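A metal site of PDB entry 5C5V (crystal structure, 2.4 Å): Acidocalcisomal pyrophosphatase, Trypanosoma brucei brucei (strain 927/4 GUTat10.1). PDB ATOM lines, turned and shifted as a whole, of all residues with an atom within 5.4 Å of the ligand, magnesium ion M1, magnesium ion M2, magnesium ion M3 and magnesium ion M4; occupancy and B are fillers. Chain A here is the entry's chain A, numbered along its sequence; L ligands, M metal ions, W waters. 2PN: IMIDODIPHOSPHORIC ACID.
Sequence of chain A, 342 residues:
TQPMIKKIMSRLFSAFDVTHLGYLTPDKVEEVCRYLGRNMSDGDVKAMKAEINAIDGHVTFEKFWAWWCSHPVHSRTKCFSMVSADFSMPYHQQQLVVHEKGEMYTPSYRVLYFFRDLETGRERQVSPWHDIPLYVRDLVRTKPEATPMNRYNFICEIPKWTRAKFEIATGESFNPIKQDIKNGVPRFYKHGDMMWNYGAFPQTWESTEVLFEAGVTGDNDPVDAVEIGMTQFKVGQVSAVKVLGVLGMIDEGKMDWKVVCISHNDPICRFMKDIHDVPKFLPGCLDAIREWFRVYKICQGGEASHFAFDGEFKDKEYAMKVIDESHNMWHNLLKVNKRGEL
The side-chain hydroxyl (OH) of Tyr 296 lies within hydrogen-bond range of an oxygen (O3) of the ligand (2.6 Å).
The side-chain hydroxyl (OH) of Tyr 198 lies close to an oxygen (O6) of the ligand (2.6 Å).
An oxygen (O3) of the ligand lies within salt-bridge range of the guanidinium group of Arg 187 (2.8 Å).
NZ of Lys 297 lies within salt-bridge range of O3 of the ligand.
The side-chain amino group (NZ) of Lys 165 sits close to an oxygen (O6) of the ligand (3.3 Å).
The side-chain amino group (NZ) of Lys 258 lies within hydrogen-bond range of the backbone carbonyl oxygen (O) of Asp 256, at 3.1 Å.
The backbone NH (N) of Asp 256 is in hydrogen-bond range of the backbone carbonyl oxygen (O) of Met 249.
N of Asp 221 sits at hydrogen-bond distance from OD2 of Asp 219, 3.2 Å away.
The side-chain carboxylate of Glu 167 sits close to the guanidinium group of Arg 187 (3.96 Å).
The side-chain amino group (NZ) of Lys 165 lies close to the side-chain carboxylate (OE2) of Glu 167, at 2.8 Å.
OD2 of Asp 180 lies within salt-bridge range of NH1 of Arg 187, at 2.9 Å.
NZ of Lys 297 lies within salt-bridge range of OE2 of Glu 252 (3.3 Å).
The backbone carbonyl oxygen (O) of Lys 165 is in hydrogen-bond range of the backbone NH (N) of Asp 180, 3.0 Å away.
The side-chain carboxylate (OD2) of Asp 221 sits close to an oxygen (O4) of the ligand.
Hydrophobic or aromatic side chains that line the ligand: Tyr 198 and Tyr 296.
11 residues have an atom within 4 Å of the ligand: Lys 165, Glu 167, Arg 187, Tyr 198, Asp 219, Asp 221, Asp 224, Asp 251, Asp 256, Tyr 296 and Lys 297.
Along chain A the residues within 4 Å of the ligand span positions 165 to 297.
Of the 20 residues printed, 3 come within 4 Å of magnesium ion M2.
Along chain A the residues within 4 Å of magnesium ion M2 span positions 219 to 256.
The nearest printed residue that does not touch magnesium ion M2 is Lys 258 (4.03 Å).
Merely in contact with magnesium ion M3: Lys 165.
The nearest printed residue that does not touch magnesium ion M3 is Arg 187 (4.004 Å).
OH of Tyr 198 touches magnesium ion M4, at 3.8 Å.
Along chain A the residues within 4 Å of magnesium ion M4 span positions 198 to 224.
The nearest printed residue that does not touch magnesium ion M4 is Pro 222 (4.2 Å).
Magnesium ion M1 is bound by water W10 (1.9 Å), the side-chain carboxylate of Asp 224 (2.0 Å), the side-chain carboxylate of Asp 256 (2.0 Å), an oxygen (O5) of the ligand (2.1 Å), the side-chain carboxylate of Asp 219 (2.2 Å) and water W2 (2.2 Å).
Magnesium ion M1 has six donor atoms within binding distance.
Magnesium ion M2 is bound by OD2 of Asp 256, 2.0 Å away.
Magnesium ion M2 is bound by water W7, at 2.1 Å.
Magnesium ion M2 is bound by an oxygen (O2) of the ligand (2.1 Å).
Water W5 binds magnesium ion M2, at 2.2 Å.
OD2 of Asp 251 is bound to magnesium ion M2 (2.3 Å).
Magnesium ion M2 is bound by O5 of the ligand.
Magnesium ion M3 is bound by water W4 (2.0 Å), water W6 (2.1 Å), O1 of the ligand (2.1 Å), water W3 (2.2 Å), OE2 of Glu 167 (2.2 Å) and O4 of the ligand (2.4 Å).
Magnesium ion M3 has six donor atoms within binding distance.
O6 of the ligand binds magnesium ion M4, 1.9 Å away.
OD1 of Asp 224 is bound to magnesium ion M4, at 2.0 Å.
Water W10 binds magnesium ion M4, at 2.1 Å.
Water W1 is bound to magnesium ion M4, at 2.1 Å.
Magnesium ion M4 is bound by water W8 (2.3 Å).
Water W9 binds magnesium ion M4 (2.3 Å).
Water W2 bridges the side-chain carboxylate (OD2) of Asp 219 (2.7 Å) and the backbone carbonyl oxygen (O) of Pro 222 (2.9 Å).
Water W7 lies within hydrogen-bond range of the side-chain hydroxyl of Tyr 296, a nitrogen (N1) of the ligand and the side-chain amino group of Lys 258.
Water W3 bridges the side-chain carboxylate (OD2) of Asp 221 and the side-chain carboxylate (OE1) of Glu 167.
Water W1 lies within hydrogen-bond range of the side-chain carboxylate of Glu 157 (2.7 Å) and the backbone carbonyl oxygen of Gly 199 (3.3 Å).
Water W11 lies within hydrogen-bond range of N1 of the ligand (2.8 Å) and OH of Tyr 189 (2.8 Å).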
ATOM      1  N   GLU A 157     -24.406 -26.227 -29.282  1.00  0.00           N
ATOM      2  CA  GLU A 157     -25.724 -25.598 -29.384  1.00  0.00           C
ATOM      3  C   GLU A 157     -25.738 -24.613 -30.564  1.00  0.00           C
ATOM      4  O   GLU A 157     -26.722 -24.521 -31.310  1.00  0.00           O
ATOM      5  CB  GLU A 157     -26.064 -24.880 -28.081  1.00  0.00           C
ATOM      6  CG  GLU A 157     -26.137 -25.826 -26.882  1.00  0.00           C
ATOM      7  CD  GLU A 157     -26.160 -25.135 -25.527  1.00  0.00           C
ATOM      8  OE1 GLU A 157     -25.475 -24.090 -25.360  1.00  0.00           O
ATOM      9  OE2 GLU A 157     -26.855 -25.654 -24.615  1.00  0.00           O
ATOM     10  N   LYS A 165     -29.877 -18.707 -31.461  1.00  0.00           N
ATOM     11  CA  LYS A 165     -29.421 -19.025 -30.108  1.00  0.00           C
ATOM     12  C   LYS A 165     -30.110 -20.272 -29.544  1.00  0.00           C
ATOM     13  O   LYS A 165     -31.021 -20.183 -28.728  1.00  0.00           O
ATOM     14  CB  LYS A 165     -29.631 -17.825 -29.192  1.00  0.00           C
ATOM     15  CG  LYS A 165     -28.500 -17.594 -28.192  1.00  0.00           C
ATOM     16  CD  LYS A 165     -28.476 -18.624 -27.083  1.00  0.00           C
ATOM     17  CE  LYS A 165     -27.359 -18.353 -26.071  1.00  0.00           C
ATOM     18  NZ  LYS A 165     -27.299 -19.392 -24.991  1.00  0.00           N
ATOM     19  N   GLU A 167     -30.220 -23.660 -27.238  1.00  0.00           N
ATOM     20  CA  GLU A 167     -29.874 -23.912 -25.842  1.00  0.00           C
ATOM     21  C   GLU A 167     -30.449 -25.276 -25.437  1.00  0.00           C
ATOM     22  O   GLU A 167     -31.538 -25.646 -25.868  1.00  0.00           O
ATOM     23  CB  GLU A 167     -30.462 -22.859 -24.907  1.00  0.00           C
ATOM     24  CG  GLU A 167     -29.695 -21.558 -24.790  1.00  0.00           C
ATOM     25  CD  GLU A 167     -30.300 -20.599 -23.753  1.00  0.00           C
ATOM     26  OE1 GLU A 167     -31.296 -20.991 -23.088  1.00  0.00           O
ATOM     27  OE2 GLU A 167     -29.781 -19.463 -23.611  1.00  0.00           O
ATOM     28  N   ASP A 180     -33.787 -20.477 -27.745  1.00  0.00           N
ATOM     29  CA  ASP A 180     -34.146 -19.557 -26.693  1.00  0.00           C
ATOM     30  C   ASP A 180     -35.159 -18.524 -27.221  1.00  0.00           C
ATOM     31  O   ASP A 180     -35.180 -18.218 -28.411  1.00  0.00           O
ATOM     32  CB  ASP A 180     -32.886 -18.872 -26.161  1.00  0.00           C
ATOM     33  CG  ASP A 180     -33.125 -18.112 -24.879  1.00  0.00           C
ATOM     34  OD1 ASP A 180     -34.168 -18.351 -24.228  1.00  0.00           O
ATOM     35  OD2 ASP A 180     -32.255 -17.284 -24.519  1.00  0.00           O
ATOM     36  N   ARG A 187     -34.960 -16.369 -30.475  1.00  0.00           N
ATOM     37  CA  ARG A 187     -33.836 -15.444 -30.321  1.00  0.00           C
ATOM     38  C   ARG A 187     -32.703 -15.641 -31.331  1.00  0.00           C
ATOM     39  O   ARG A 187     -32.176 -16.744 -31.506  1.00  0.00           O
ATOM     40  CB  ARG A 187     -33.293 -15.536 -28.894  1.00  0.00           C
ATOM     41  CG  ARG A 187     -32.036 -14.757 -28.599  1.00  0.00           C
ATOM     42  CD  ARG A 187     -31.533 -15.078 -27.193  1.00  0.00           C
ATOM     43  NE  ARG A 187     -30.300 -14.377 -26.833  1.00  0.00           N
ATOM     44  CZ  ARG A 187     -29.501 -14.729 -25.828  1.00  0.00           C
ATOM     45  NH1 ARG A 187     -29.779 -15.787 -25.080  1.00  0.00           N
ATOM     46  NH2 ARG A 187     -28.409 -14.022 -25.577  1.00  0.00           N
ATOM     47  N   TYR A 189     -28.889 -13.721 -32.209  1.00  0.00           N
ATOM     48  CA  TYR A 189     -27.938 -12.702 -31.785  1.00  0.00           C
ATOM     49  C   TYR A 189     -28.094 -11.458 -32.649  1.00  0.00           C
ATOM     50  O   TYR A 189     -28.067 -11.536 -33.881  1.00  0.00           O
ATOM     51  CB  TYR A 189     -26.507 -13.193 -31.895  1.00  0.00           C
ATOM     52  CG  TYR A 189     -26.104 -14.214 -30.880  1.00  0.00           C
ATOM     53  CD1 TYR A 189     -26.460 -14.078 -29.542  1.00  0.00           C
ATOM     54  CD2 TYR A 189     -25.321 -15.290 -31.247  1.00  0.00           C
ATOM     55  CE1 TYR A 189     -26.065 -15.007 -28.621  1.00  0.00           C
ATOM     56  CE2 TYR A 189     -24.919 -16.230 -30.332  1.00  0.00           C
ATOM     57  CZ  TYR A 189     -25.295 -16.077 -29.026  1.00  0.00           C
ATOM     58  OH  TYR A 189     -24.881 -17.010 -28.094  1.00  0.00           O
ATOM     59  N   TYR A 198     -20.204 -22.844 -30.270  1.00  0.00           N
ATOM     60  CA  TYR A 198     -20.597 -22.513 -28.929  1.00  0.00           C
ATOM     61  C   TYR A 198     -21.579 -23.546 -28.384  1.00  0.00           C
ATOM     62  O   TYR A 198     -22.419 -24.050 -29.113  1.00  0.00           O
ATOM     63  CB  TYR A 198     -21.228 -21.122 -28.906  1.00  0.00           C
ATOM     64  CG  TYR A 198     -21.634 -20.647 -27.542  1.00  0.00           C
ATOM     65  CD1 TYR A 198     -20.699 -20.096 -26.669  1.00  0.00           C
ATOM     66  CD2 TYR A 198     -22.943 -20.768 -27.103  1.00  0.00           C
ATOM     67  CE1 TYR A 198     -21.066 -19.670 -25.407  1.00  0.00           C
ATOM     68  CE2 TYR A 198     -23.315 -20.348 -25.834  1.00  0.00           C
ATOM     69  CZ  TYR A 198     -22.380 -19.790 -25.005  1.00  0.00           C
ATOM     70  OH  TYR A 198     -22.749 -19.370 -23.750  1.00  0.00           O
ATOM     71  N   GLY A 199     -21.459 -23.874 -27.102  1.00  0.00           N
ATOM     72  CA  GLY A 199     -22.339 -24.859 -26.507  1.00  0.00           C
ATOM     73  C   GLY A 199     -22.111 -25.040 -25.018  1.00  0.00           C
ATOM     74  O   GLY A 199     -21.871 -24.080 -24.296  1.00  0.00           O
ATOM     75  N   ALA A 200     -22.162 -26.286 -24.559  1.00  0.00           N
ATOM     76  CA  ALA A 200     -22.100 -26.550 -23.143  1.00  0.00           C
ATOM     77  C   ALA A 200     -21.475 -27.903 -22.834  1.00  0.00           C
ATOM     78  O   ALA A 200     -21.369 -28.770 -23.705  1.00  0.00           O
ATOM     79  CB  ALA A 200     -23.491 -26.459 -22.535  1.00  0.00           C
ATOM     80  N   ASP A 219     -25.220 -18.897 -13.265  1.00  0.00           N
ATOM     81  CA  ASP A 219     -26.312 -18.477 -14.142  1.00  0.00           C
ATOM     82  C   ASP A 219     -27.336 -19.590 -14.359  1.00  0.00           C
ATOM     83  O   ASP A 219     -28.175 -19.503 -15.255  1.00  0.00           O
ATOM     84  CB  ASP A 219     -25.770 -17.961 -15.498  1.00  0.00           C
ATOM     85  CG  ASP A 219     -25.457 -19.094 -16.492  1.00  0.00           C
ATOM     86  OD1 ASP A 219     -25.535 -18.810 -17.701  1.00  0.00           O
ATOM     87  OD2 ASP A 219     -25.148 -20.248 -16.070  1.00  0.00           O
ATOM     88  N   ASP A 221     -27.238 -22.640 -15.471  1.00  0.00           N
ATOM     89  CA  ASP A 221     -27.129 -23.377 -16.737  1.00  0.00           C
ATOM     90  C   ASP A 221     -25.921 -24.292 -16.722  1.00  0.00           C
ATOM     91  O   ASP A 221     -25.023 -24.131 -15.902  1.00  0.00           O
ATOM     92  CB  ASP A 221     -27.026 -22.417 -17.929  1.00  0.00           C
ATOM     93  CG  ASP A 221     -28.346 -22.161 -18.632  1.00  0.00           C
ATOM     94  OD1 ASP A 221     -29.152 -23.107 -18.779  1.00  0.00           O
ATOM     95  OD2 ASP A 221     -28.589 -21.026 -19.084  1.00  0.00           O
ATOM     96  N   PRO A 222     -25.875 -25.256 -17.645  1.00  0.00           N
ATOM     97  CA  PRO A 222     -24.621 -25.999 -17.811  1.00  0.00           C
ATOM     98  C   PRO A 222     -23.460 -25.040 -18.103  1.00  0.00           C
ATOM     99  O   PRO A 222     -23.693 -23.949 -18.626  1.00  0.00           O
ATOM    100  CB  PRO A 222     -24.902 -26.907 -19.011  1.00  0.00           C
ATOM    101  CG  PRO A 222     -26.363 -27.037 -19.038  1.00  0.00           C
ATOM    102  CD  PRO A 222     -26.919 -25.747 -18.561  1.00  0.00           C
ATOM    103  N   ASP A 224     -20.600 -23.185 -19.949  1.00  0.00           N
ATOM    104  CA  ASP A 224     -20.512 -22.788 -21.352  1.00  0.00           C
ATOM    105  C   ASP A 224     -19.125 -23.031 -21.920  1.00  0.00           C
ATOM    106  O   ASP A 224     -18.120 -22.837 -21.243  1.00  0.00           O
ATOM    107  CB  ASP A 224     -20.897 -21.318 -21.493  1.00  0.00           C
ATOM    108  CG  ASP A 224     -22.353 -21.039 -21.126  1.00  0.00           C
ATOM    109  OD1 ASP A 224     -23.227 -21.855 -21.493  1.00  0.00           O
ATOM    110  OD2 ASP A 224     -22.610 -20.021 -20.470  1.00  0.00           O
ATOM    111  N   MET A 249     -16.381 -14.749 -17.103  1.00  0.00           N
ATOM    112  CA  MET A 249     -17.476 -13.857 -17.413  1.00  0.00           C
ATOM    113  C   MET A 249     -18.528 -13.810 -16.310  1.00  0.00           C
ATOM    114  O   MET A 249     -19.019 -14.866 -15.865  1.00  0.00           O
ATOM    115  CB  MET A 249     -18.132 -14.285 -18.723  1.00  0.00           C
ATOM    116  CG  MET A 249     -19.345 -13.461 -19.117  1.00  0.00           C
ATOM    117  SD  MET A 249     -19.968 -14.006 -20.719  1.00  0.00           S
ATOM    118  CE  MET A 249     -21.404 -12.934 -20.908  1.00  0.00           C
ATOM    119  N   ASP A 251     -22.243 -12.475 -16.030  1.00  0.00           N
ATOM    120  CA  ASP A 251     -23.302 -12.092 -16.950  1.00  0.00           C
ATOM    121  C   ASP A 251     -24.590 -11.744 -16.193  1.00  0.00           C
ATOM    122  O   ASP A 251     -25.197 -12.626 -15.581  1.00  0.00           O
ATOM    123  CB  ASP A 251     -23.543 -13.242 -17.952  1.00  0.00           C
ATOM    124  CG  ASP A 251     -24.535 -12.882 -19.040  1.00  0.00           C
ATOM    125  OD1 ASP A 251     -25.004 -11.726 -19.061  1.00  0.00           O
ATOM    126  OD2 ASP A 251     -24.843 -13.759 -19.883  1.00  0.00           O
ATOM    127  N   GLU A 252     -24.999 -10.474 -16.228  1.00  0.00           N
ATOM    128  CA  GLU A 252     -26.214 -10.056 -15.504  1.00  0.00           C
ATOM    129  C   GLU A 252     -26.182 -10.467 -14.032  1.00  0.00           C
ATOM    130  O   GLU A 252     -27.178 -10.934 -13.478  1.00  0.00           O
ATOM    131  CB  GLU A 252     -27.471 -10.647 -16.185  1.00  0.00           C
ATOM    132  CG  GLU A 252     -27.727 -10.138 -17.607  1.00  0.00           C
ATOM    133  CD  GLU A 252     -28.508 -11.140 -18.486  1.00  0.00           C
ATOM    134  OE1 GLU A 252     -28.682 -12.315 -18.087  1.00  0.00           O
ATOM    135  OE2 GLU A 252     -28.954 -10.765 -19.590  1.00  0.00           O
ATOM    136  N   ASP A 256     -20.633 -16.961 -15.015  1.00  0.00           N
ATOM    137  CA  ASP A 256     -20.937 -17.494 -16.327  1.00  0.00           C
ATOM    138  C   ASP A 256     -19.646 -17.813 -17.068  1.00  0.00           C
ATOM    139  O   ASP A 256     -19.401 -17.294 -18.169  1.00  0.00           O
ATOM    140  CB  ASP A 256     -21.796 -16.499 -17.098  1.00  0.00           C
ATOM    141  CG  ASP A 256     -22.629 -17.140 -18.161  1.00  0.00           C
ATOM    142  OD1 ASP A 256     -22.777 -18.392 -18.134  1.00  0.00           O
ATOM    143  OD2 ASP A 256     -23.154 -16.407 -19.027  1.00  0.00           O
ATOM    144  N   LYS A 258     -16.693 -19.077 -19.240  1.00  0.00           N
ATOM    145  CA  LYS A 258     -16.626 -19.440 -20.651  1.00  0.00           C
ATOM    146  C   LYS A 258     -15.348 -20.227 -20.893  1.00  0.00           C
ATOM    147  O   LYS A 258     -14.259 -19.657 -20.934  1.00  0.00           O
ATOM    148  CB  LYS A 258     -16.669 -18.193 -21.534  1.00  0.00           C
ATOM    149  CG  LYS A 258     -17.980 -17.420 -21.466  1.00  0.00           C
ATOM    150  CD  LYS A 258     -19.077 -18.113 -22.253  1.00  0.00           C
ATOM    151  CE  LYS A 258     -20.381 -17.327 -22.182  1.00  0.00           C
ATOM    152  NZ  LYS A 258     -20.967 -17.365 -20.817  1.00  0.00           N
ATOM    153  N   TYR A 296     -21.852  -8.130 -26.463  1.00  0.00           N
ATOM    154  CA  TYR A 296     -22.886  -8.609 -27.391  1.00  0.00           C
ATOM    155  C   TYR A 296     -24.325  -8.288 -26.984  1.00  0.00           C
ATOM    156  O   TYR A 296     -25.175  -8.167 -27.838  1.00  0.00           O
ATOM    157  CB  TYR A 296     -22.737 -10.125 -27.640  1.00  0.00           C
ATOM    158  CG  TYR A 296     -23.167 -11.081 -26.531  1.00  0.00           C
ATOM    159  CD1 TYR A 296     -24.191 -11.998 -26.744  1.00  0.00           C
ATOM    160  CD2 TYR A 296     -22.521 -11.105 -25.298  1.00  0.00           C
ATOM    161  CE1 TYR A 296     -24.584 -12.910 -25.742  1.00  0.00           C
ATOM    162  CE2 TYR A 296     -22.911 -11.989 -24.280  1.00  0.00           C
ATOM    163  CZ  TYR A 296     -23.930 -12.905 -24.521  1.00  0.00           C
ATOM    164  OH  TYR A 296     -24.305 -13.775 -23.543  1.00  0.00           O
ATOM    165  N   LYS A 297     -24.589  -8.114 -25.698  1.00  0.00           N
ATOM    166  CA  LYS A 297     -25.965  -7.841 -25.271  1.00  0.00           C
ATOM    167  C   LYS A 297     -26.304  -6.351 -25.221  1.00  0.00           C
ATOM    168  O   LYS A 297     -27.466  -5.983 -25.051  1.00  0.00           O
ATOM    169  CB  LYS A 297     -26.237  -8.473 -23.898  1.00  0.00           C
ATOM    170  CG  LYS A 297     -26.353 -10.006 -23.935  1.00  0.00           C
ATOM    171  CD  LYS A 297     -26.590 -10.590 -22.531  1.00  0.00           C
ATOM    172  CE  LYS A 297     -26.604 -12.126 -22.555  1.00  0.00           C
ATOM    173  NZ  LYS A 297     -26.898 -12.748 -21.222  1.00  0.00           N
HETATM  174  P1  2PN L   1     -26.762 -16.106 -22.751  1.00  0.00           P
HETATM  175  O1  2PN L   1     -28.279 -16.426 -22.721  1.00  0.00           O
HETATM  176  O2  2PN L   1     -26.365 -15.514 -21.368  1.00  0.00           O
HETATM  177  O3  2PN L   1     -26.465 -15.159 -23.946  1.00  0.00           O
HETATM  178  N1  2PN L   1     -25.940 -17.485 -23.052  1.00  0.00           N
HETATM  179  P2  2PN L   1     -25.785 -18.724 -21.985  1.00  0.00           P
HETATM  180  O4  2PN L   1     -27.183 -19.206 -21.479  1.00  0.00           O
HETATM  181  O5  2PN L   1     -24.986 -18.203 -20.809  1.00  0.00           O
HETATM  182  O6  2PN L   1     -25.090 -19.840 -22.632  1.00  0.00           O
HETATM  183 MG    MG M   1     -24.121 -19.363 -19.311  1.00  0.00          MG
HETATM  184 MG    MG M   2     -24.704 -15.999 -20.209  1.00  0.00          MG
HETATM  185 MG    MG M   3     -29.252 -18.155 -21.895  1.00  0.00          MG
HETATM  186 MG    MG M   4     -25.149 -21.432 -21.625  1.00  0.00          MG
HETATM  187  O   HOH W   1     -24.668 -22.704 -23.187  1.00  0.00           O
HETATM  188  O   HOH W   2     -23.611 -21.142 -18.096  1.00  0.00           O
HETATM  189  O   HOH W   3     -30.380 -19.691 -20.764  1.00  0.00           O
HETATM  190  O   HOH W   4     -30.981 -17.068 -21.928  1.00  0.00           O
HETATM  191  O   HOH W   5     -26.151 -16.324 -18.539  1.00  0.00           O
HETATM  192  O   HOH W   6     -29.276 -17.003 -20.132  1.00  0.00           O
HETATM  193  O   HOH W   7     -23.525 -15.818 -21.916  1.00  0.00           O
HETATM  194  O   HOH W   8     -27.278 -21.874 -22.239  1.00  0.00           O
HETATM  195  O   HOH W   9     -25.319 -23.519 -20.625  1.00  0.00           O
HETATM  196  O   HOH W  10     -25.598 -20.471 -19.862  1.00  0.00           O
HETATM  197  O   HOH W  11     -24.528 -16.789 -25.327  1.00  0.00           O
